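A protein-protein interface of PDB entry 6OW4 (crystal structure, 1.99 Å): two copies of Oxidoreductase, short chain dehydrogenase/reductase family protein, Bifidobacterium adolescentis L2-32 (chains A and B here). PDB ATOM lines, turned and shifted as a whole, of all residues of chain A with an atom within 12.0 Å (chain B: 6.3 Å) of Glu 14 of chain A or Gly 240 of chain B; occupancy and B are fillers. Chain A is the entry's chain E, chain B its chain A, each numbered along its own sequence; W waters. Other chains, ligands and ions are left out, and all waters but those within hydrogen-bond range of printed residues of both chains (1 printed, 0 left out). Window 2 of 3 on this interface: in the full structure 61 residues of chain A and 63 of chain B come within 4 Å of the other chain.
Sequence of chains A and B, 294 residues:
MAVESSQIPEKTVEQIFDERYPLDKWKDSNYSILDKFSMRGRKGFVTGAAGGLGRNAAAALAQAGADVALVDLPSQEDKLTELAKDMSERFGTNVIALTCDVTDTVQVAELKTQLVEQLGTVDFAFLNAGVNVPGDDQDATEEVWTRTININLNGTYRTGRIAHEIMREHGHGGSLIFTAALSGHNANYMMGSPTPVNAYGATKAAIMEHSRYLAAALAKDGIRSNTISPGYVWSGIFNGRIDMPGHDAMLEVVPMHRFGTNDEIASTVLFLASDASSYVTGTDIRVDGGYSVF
Of the 7 printed residues of chain B, 4 touch a printed residue of chain A. Of the 13 printed residues of chain A, 4 touch a printed residue of chain B. Among the printed residues, 7 pairs touch across the chains. Among the printed residues, no Asp or Glu carboxylate lies within 4 Å of a Lys or Arg side-chain nitrogen of the other chain.
The backbone carbonyl oxygen (O) of Gly 236 of chain B sits close to the side-chain amide oxygen (OD1) of Asn 239 of chain B (3.1 Å). The side-chain amide oxygen (OD1) of Asn 239 of chain B sits at hydrogen-bond distance from the indole nitrogen (NE1) of Trp 234 of chain B.
No position is printed for both chains.
N of Gly 240 of chain B lies within hydrogen-bond range of OE1 of Glu 14 of chain A (3.0 Å).
Glu 14 of chain A touches just these residues of chain B: Trp 234 (3.6 Å), Asn 239 (3.6 Å) and Gly 240 (3.0 Å). Gln 15 of chain A touches none of the printed residues of chain B. Of the printed residues of chain B, Phe 17 of chain A touches Trp 234 and Ile 242. Printed residues of chain B within 4 Å of Tyr 21 of chain A: Trp 234 (3.3 Å). Printed residues of chain B within 4 Å of Leu 23 of chain A: Trp 234. Of the printed residues of chain A, Trp 234 of chain B touches Glu 14, Phe 17, Tyr 21 and Leu 23. Asn 239 of chain B touches one residue of chain A. Printed residues of chain A within 4 Å of Gly 240 of chain B: Glu 14. No residue of chain A comes within 4 Å of Arg 241 of chain B. The nearest residue of chain B that does not touch Glu 14 of chain A is Ile 242 of chain B (4.6 Å). The nearest residue of chain A that does not touch Gly 240 of chain B is Phe 17 of chain A (6.1 Å).
Among the printed residues, merely in contact across the chains: Glu 14 of chain A with Trp 234 of chain B (3.6 Å), Glu 14 of chain A with Asn 239 of chain B (3.6 Å), Phe 17 of chain A with Trp 234 of chain B (3.6 Å), Phe 17 of chain A with Ile 242 of chain B (3.7 Å), Tyr 21 of chain A with Trp 234 of chain B (3.3 Å) and Leu 23 of chain A with Trp 234 of chain B (3.8 Å).
Water W1 lies within hydrogen-bond range of the backbone carbonyl oxygen (O) of Trp 234 of chain B (2.6 Å) and the backbone carbonyl oxygen (O) of Pro 22 of chain A (2.7 Å).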
ATOM      1  N   LYS A  11     -34.917 -36.028  15.646  1.00  0.00           N
ATOM      2  CA  LYS A  11     -34.344 -36.718  14.443  1.00  0.00           C
ATOM      3  C   LYS A  11     -33.280 -35.827  13.782  1.00  0.00           C
ATOM      4  O   LYS A  11     -32.269 -36.386  13.317  1.00  0.00           O
ATOM      5  CB  LYS A  11     -35.461 -37.122  13.472  1.00  0.00           C
ATOM      6  CG  LYS A  11     -36.145 -35.983  12.726  1.00  0.00           C
ATOM      7  CD  LYS A  11     -37.611 -36.238  12.436  1.00  0.00           C
ATOM      8  CE  LYS A  11     -37.874 -37.560  11.745  1.00  0.00           C
ATOM      9  NZ  LYS A  11     -39.320 -37.753  11.479  1.00  0.00           N
ATOM     10  N   THR A  12     -33.494 -34.505  13.740  1.00  0.00           N
ATOM     11  CA  THR A  12     -32.473 -33.497  13.339  1.00  0.00           C
ATOM     12  C   THR A  12     -31.434 -33.392  14.462  1.00  0.00           C
ATOM     13  O   THR A  12     -31.819 -33.578  15.634  1.00  0.00           O
ATOM     14  CB  THR A  12     -33.103 -32.128  13.043  1.00  0.00           C
ATOM     15  OG1 THR A  12     -34.273 -32.327  12.249  1.00  0.00           O
ATOM     16  CG2 THR A  12     -32.161 -31.188  12.323  1.00  0.00           C
ATOM     17  N   VAL A  13     -30.174 -33.115  14.114  1.00  0.00           N
ATOM     18  CA  VAL A  13     -29.044 -32.976  15.085  1.00  0.00           C
ATOM     19  C   VAL A  13     -29.415 -31.912  16.127  1.00  0.00           C
ATOM     20  O   VAL A  13     -29.130 -32.131  17.317  1.00  0.00           O
ATOM     21  CB  VAL A  13     -27.706 -32.648  14.389  1.00  0.00           C
ATOM     22  CG1 VAL A  13     -27.233 -33.797  13.513  1.00  0.00           C
ATOM     23  CG2 VAL A  13     -27.756 -31.353  13.587  1.00  0.00           C
ATOM     24  N   GLU A  14     -30.047 -30.816  15.689  1.00  0.00           N
ATOM     25  CA  GLU A  14     -30.416 -29.654  16.541  1.00  0.00           C
ATOM     26  C   GLU A  14     -31.606 -30.023  17.436  1.00  0.00           C
ATOM     27  O   GLU A  14     -31.636 -29.540  18.583  1.00  0.00           O
ATOM     28  CB  GLU A  14     -30.730 -28.430  15.677  1.00  0.00           C
ATOM     29  CG  GLU A  14     -30.673 -27.120  16.445  1.00  0.00           C
ATOM     30  CD  GLU A  14     -29.320 -26.796  17.062  1.00  0.00           C
ATOM     31  OE1 GLU A  14     -28.291 -26.991  16.378  1.00  0.00           O
ATOM     32  OE2 GLU A  14     -29.297 -26.358  18.228  1.00  0.00           O
ATOM     33  N   GLN A  15     -32.542 -30.837  16.934  1.00  0.00           N
ATOM     34  CA  GLN A  15     -33.706 -31.355  17.705  1.00  0.00           C
ATOM     35  C   GLN A  15     -33.209 -32.219  18.873  1.00  0.00           C
ATOM     36  O   GLN A  15     -33.833 -32.159  19.952  1.00  0.00           O
ATOM     37  CB  GLN A  15     -34.655 -32.153  16.806  1.00  0.00           C
ATOM     38  CG  GLN A  15     -35.484 -31.285  15.866  1.00  0.00           C
ATOM     39  CD  GLN A  15     -36.506 -32.063  15.069  1.00  0.00           C
ATOM     40  OE1 GLN A  15     -37.278 -31.497  14.298  1.00  0.00           O
ATOM     41  NE2 GLN A  15     -36.529 -33.374  15.249  1.00  0.00           N
ATOM     42  N   ILE A  16     -32.133 -32.988  18.667  1.00  0.00           N
ATOM     43  CA  ILE A  16     -31.520 -33.865  19.711  1.00  0.00           C
ATOM     44  C   ILE A  16     -30.874 -32.978  20.782  1.00  0.00           C
ATOM     45  O   ILE A  16     -31.071 -33.270  21.977  1.00  0.00           O
ATOM     46  CB  ILE A  16     -30.505 -34.859  19.104  1.00  0.00           C
ATOM     47  CG1 ILE A  16     -31.160 -35.799  18.087  1.00  0.00           C
ATOM     48  CG2 ILE A  16     -29.795 -35.639  20.203  1.00  0.00           C
ATOM     49  CD1 ILE A  16     -30.173 -36.527  17.202  1.00  0.00           C
ATOM     50  N   PHE A  17     -30.125 -31.950  20.369  1.00  0.00           N
ATOM     51  CA  PHE A  17     -29.469 -30.964  21.272  1.00  0.00           C
ATOM     52  C   PHE A  17     -30.529 -30.211  22.086  1.00  0.00           C
ATOM     53  O   PHE A  17     -30.290 -29.961  23.279  1.00  0.00           O
ATOM     54  CB  PHE A  17     -28.599 -29.973  20.490  1.00  0.00           C
ATOM     55  CG  PHE A  17     -27.337 -30.531  19.873  1.00  0.00           C
ATOM     56  CD1 PHE A  17     -26.582 -31.499  20.521  1.00  0.00           C
ATOM     57  CD2 PHE A  17     -26.881 -30.053  18.652  1.00  0.00           C
ATOM     58  CE1 PHE A  17     -25.419 -31.996  19.947  1.00  0.00           C
ATOM     59  CE2 PHE A  17     -25.716 -30.548  18.082  1.00  0.00           C
ATOM     60  CZ  PHE A  17     -24.989 -31.519  18.729  1.00  0.00           C
ATOM     61  N   ASP A  18     -31.658 -29.855  21.461  1.00  0.00           N
ATOM     62  CA  ASP A  18     -32.780 -29.117  22.107  1.00  0.00           C
ATOM     63  C   ASP A  18     -33.390 -29.987  23.213  1.00  0.00           C
ATOM     64  O   ASP A  18     -33.784 -29.425  24.255  1.00  0.00           O
ATOM     65  CB  ASP A  18     -33.843 -28.697  21.087  1.00  0.00           C
ATOM     66  CG  ASP A  18     -33.354 -27.716  20.033  1.00  0.00           C
ATOM     67  OD1 ASP A  18     -32.284 -27.110  20.240  1.00  0.00           O
ATOM     68  OD2 ASP A  18     -34.042 -27.575  19.001  1.00  0.00           O
ATOM     69  N   GLU A  19     -33.460 -31.304  22.993  1.00  0.00           N
ATOM     70  CA  GLU A  19     -34.018 -32.290  23.957  1.00  0.00           C
ATOM     71  C   GLU A  19     -32.976 -32.611  25.038  1.00  0.00           C
ATOM     72  O   GLU A  19     -33.373 -32.758  26.207  1.00  0.00           O
ATOM     73  CB  GLU A  19     -34.476 -33.551  23.222  1.00  0.00           C
ATOM     74  CG  GLU A  19     -35.722 -33.328  22.379  1.00  0.00           C
ATOM     75  CD  GLU A  19     -36.031 -34.427  21.375  1.00  0.00           C
ATOM     76  OE1 GLU A  19     -35.087 -35.128  20.954  1.00  0.00           O
ATOM     77  OE2 GLU A  19     -37.216 -34.578  21.013  1.00  0.00           O
ATOM     78  N   ARG A  20     -31.696 -32.722  24.669  1.00  0.00           N
ATOM     79  CA  ARG A  20     -30.586 -32.997  25.621  1.00  0.00           C
ATOM     80  C   ARG A  20     -30.431 -31.821  26.592  1.00  0.00           C
ATOM     81  O   ARG A  20     -30.299 -32.072  27.805  1.00  0.00           O
ATOM     82  CB  ARG A  20     -29.266 -33.248  24.883  1.00  0.00           C
ATOM     83  CG  ARG A  20     -29.084 -34.675  24.388  1.00  0.00           C
ATOM     84  CD  ARG A  20     -27.669 -34.924  23.903  1.00  0.00           C
ATOM     85  NE  ARG A  20     -27.562 -36.147  23.118  1.00  0.00           N
ATOM     86  CZ  ARG A  20     -26.480 -36.525  22.440  1.00  0.00           C
ATOM     87  NH1 ARG A  20     -25.390 -35.776  22.440  1.00  0.00           N
ATOM     88  NH2 ARG A  20     -26.493 -37.656  21.757  1.00  0.00           N
ATOM     89  N   TYR A  21     -30.453 -30.589  26.077  1.00  0.00           N
ATOM     90  CA  TYR A  21     -30.061 -29.359  26.811  1.00  0.00           C
ATOM     91  C   TYR A  21     -31.193 -28.332  26.796  1.00  0.00           C
ATOM     92  O   TYR A  21     -31.220 -27.461  25.930  1.00  0.00           O
ATOM     93  CB  TYR A  21     -28.792 -28.772  26.188  1.00  0.00           C
ATOM     94  CG  TYR A  21     -27.646 -29.740  26.034  1.00  0.00           C
ATOM     95  CD1 TYR A  21     -27.108 -30.394  27.130  1.00  0.00           C
ATOM     96  CD2 TYR A  21     -27.077 -29.981  24.792  1.00  0.00           C
ATOM     97  CE1 TYR A  21     -26.045 -31.272  26.998  1.00  0.00           C
ATOM     98  CE2 TYR A  21     -26.015 -30.858  24.643  1.00  0.00           C
ATOM     99  CZ  TYR A  21     -25.497 -31.507  25.749  1.00  0.00           C
ATOM    100  OH  TYR A  21     -24.447 -32.368  25.613  1.00  0.00           O
ATOM    101  N   PRO A  22     -32.153 -28.387  27.752  1.00  0.00           N
ATOM    102  CA  PRO A  22     -33.145 -27.322  27.911  1.00  0.00           C
ATOM    103  C   PRO A  22     -32.480 -25.994  28.308  1.00  0.00           C
ATOM    104  O   PRO A  22     -31.524 -26.022  29.065  1.00  0.00           O
ATOM    105  CB  PRO A  22     -34.062 -27.806  29.045  1.00  0.00           C
ATOM    106  CG  PRO A  22     -33.804 -29.294  29.129  1.00  0.00           C
ATOM    107  CD  PRO A  22     -32.359 -29.481  28.712  1.00  0.00           C
ATOM    108  N   LEU A  23     -33.009 -24.880  27.795  1.00  0.00           N
ATOM    109  CA  LEU A  23     -32.422 -23.521  27.938  1.00  0.00           C
ATOM    110  C   LEU A  23     -33.066 -22.777  29.113  1.00  0.00           C
ATOM    111  O   LEU A  23     -32.338 -22.034  29.794  1.00  0.00           O
ATOM    112  CB  LEU A  23     -32.618 -22.753  26.627  1.00  0.00           C
ATOM    113  CG  LEU A  23     -31.499 -22.896  25.597  1.00  0.00           C
ATOM    114  CD1 LEU A  23     -31.113 -24.351  25.394  1.00  0.00           C
ATOM    115  CD2 LEU A  23     -31.907 -22.265  24.274  1.00  0.00           C
ATOM    116  N   TRP B 234     -24.313 -25.373  27.324  1.00  0.00           N
ATOM    117  CA  TRP B 234     -25.255 -25.217  26.185  1.00  0.00           C
ATOM    118  C   TRP B 234     -26.275 -24.125  26.528  1.00  0.00           C
ATOM    119  O   TRP B 234     -27.418 -24.467  26.896  1.00  0.00           O
ATOM    120  CB  TRP B 234     -25.932 -26.551  25.855  1.00  0.00           C
ATOM    121  CG  TRP B 234     -26.671 -26.521  24.555  1.00  0.00           C
ATOM    122  CD1 TRP B 234     -27.977 -26.182  24.350  1.00  0.00           C
ATOM    123  CD2 TRP B 234     -26.123 -26.807  23.258  1.00  0.00           C
ATOM    124  NE1 TRP B 234     -28.284 -26.256  23.018  1.00  0.00           N
ATOM    125  CE2 TRP B 234     -27.165 -26.636  22.323  1.00  0.00           C
ATOM    126  CE3 TRP B 234     -24.860 -27.197  22.802  1.00  0.00           C
ATOM    127  CZ2 TRP B 234     -26.977 -26.841  20.957  1.00  0.00           C
ATOM    128  CZ3 TRP B 234     -24.677 -27.401  21.453  1.00  0.00           C
ATOM    129  CH2 TRP B 234     -25.722 -27.225  20.546  1.00  0.00           C
ATOM    130  N   GLY B 236     -27.387 -21.525  24.591  1.00  0.00           N
ATOM    131  CA  GLY B 236     -28.079 -20.944  23.425  1.00  0.00           C
ATOM    132  C   GLY B 236     -27.076 -20.445  22.399  1.00  0.00           C
ATOM    133  O   GLY B 236     -27.444 -20.345  21.213  1.00  0.00           O
ATOM    134  N   PHE B 238     -24.345 -21.837  21.252  1.00  0.00           N
ATOM    135  CA  PHE B 238     -23.779 -22.921  20.401  1.00  0.00           C
ATOM    136  C   PHE B 238     -24.813 -23.420  19.383  1.00  0.00           C
ATOM    137  O   PHE B 238     -24.420 -24.166  18.466  1.00  0.00           O
ATOM    138  CB  PHE B 238     -23.278 -24.078  21.270  1.00  0.00           C
ATOM    139  CG  PHE B 238     -22.121 -23.725  22.169  1.00  0.00           C
ATOM    140  CD1 PHE B 238     -20.845 -23.564  21.649  1.00  0.00           C
ATOM    141  CD2 PHE B 238     -22.304 -23.556  23.533  1.00  0.00           C
ATOM    142  CE1 PHE B 238     -19.778 -23.239  22.472  1.00  0.00           C
ATOM    143  CE2 PHE B 238     -21.235 -23.230  24.355  1.00  0.00           C
ATOM    144  CZ  PHE B 238     -19.974 -23.072  23.824  1.00  0.00           C
ATOM    145  N   ASN B 239     -26.082 -23.023  19.530  1.00  0.00           N
ATOM    146  CA  ASN B 239     -27.216 -23.512  18.698  1.00  0.00           C
ATOM    147  C   ASN B 239     -26.904 -23.274  17.217  1.00  0.00           C
ATOM    148  O   ASN B 239     -26.650 -22.110  16.844  1.00  0.00           O
ATOM    149  CB  ASN B 239     -28.541 -22.851  19.084  1.00  0.00           C
ATOM    150  CG  ASN B 239     -28.983 -23.193  20.490  1.00  0.00           C
ATOM    151  OD1 ASN B 239     -28.155 -23.404  21.371  1.00  0.00           O
ATOM    152  ND2 ASN B 239     -30.285 -23.243  20.712  1.00  0.00           N
ATOM    153  N   GLY B 240     -26.895 -24.348  16.420  1.00  0.00           N
ATOM    154  CA  GLY B 240     -26.760 -24.307  14.951  1.00  0.00           C
ATOM    155  C   GLY B 240     -25.336 -24.038  14.491  1.00  0.00           C
ATOM    156  O   GLY B 240     -25.143 -23.906  13.271  1.00  0.00           O
ATOM    157  N   ARG B 241     -24.372 -23.965  15.415  1.00  0.00           N
ATOM    158  CA  ARG B 241     -22.940 -23.689  15.111  1.00  0.00           C
ATOM    159  C   ARG B 241     -22.136 -24.997  15.106  1.00  0.00           C
ATOM    160  O   ARG B 241     -21.128 -25.056  14.371  1.00  0.00           O
ATOM    161  CB  ARG B 241     -22.348 -22.691  16.112  1.00  0.00           C
ATOM    162  CG  ARG B 241     -22.401 -21.241  15.647  1.00  0.00           C
ATOM    163  CD  ARG B 241     -21.371 -20.367  16.337  1.00  0.00           C
ATOM    164  NE  ARG B 241     -21.906 -19.725  17.532  1.00  0.00           N
ATOM    165  CZ  ARG B 241     -22.285 -18.450  17.620  1.00  0.00           C
ATOM    166  NH1 ARG B 241     -22.189 -17.638  16.580  1.00  0.00           N
ATOM    167  NH2 ARG B 241     -22.758 -17.985  18.763  1.00  0.00           N
ATOM    168  N   ILE B 242     -22.552 -25.999  15.891  1.00  0.00           N
ATOM    169  CA  ILE B 242     -21.836 -27.306  16.007  1.00  0.00           C
ATOM    170  C   ILE B 242     -22.756 -28.445  15.547  1.00  0.00           C
ATOM    171  O   ILE B 242     -23.989 -28.320  15.690  1.00  0.00           O
ATOM    172  CB  ILE B 242     -21.300 -27.529  17.437  1.00  0.00           C
ATOM    173  CG1 ILE B 242     -22.405 -27.857  18.446  1.00  0.00           C
ATOM    174  CG2 ILE B 242     -20.469 -26.338  17.893  1.00  0.00           C
ATOM    175  CD1 ILE B 242     -21.902 -28.595  19.663  1.00  0.00           C
HETATM  176  O   HOH W   1     -28.954 -25.081  28.853  1.00  0.00           O
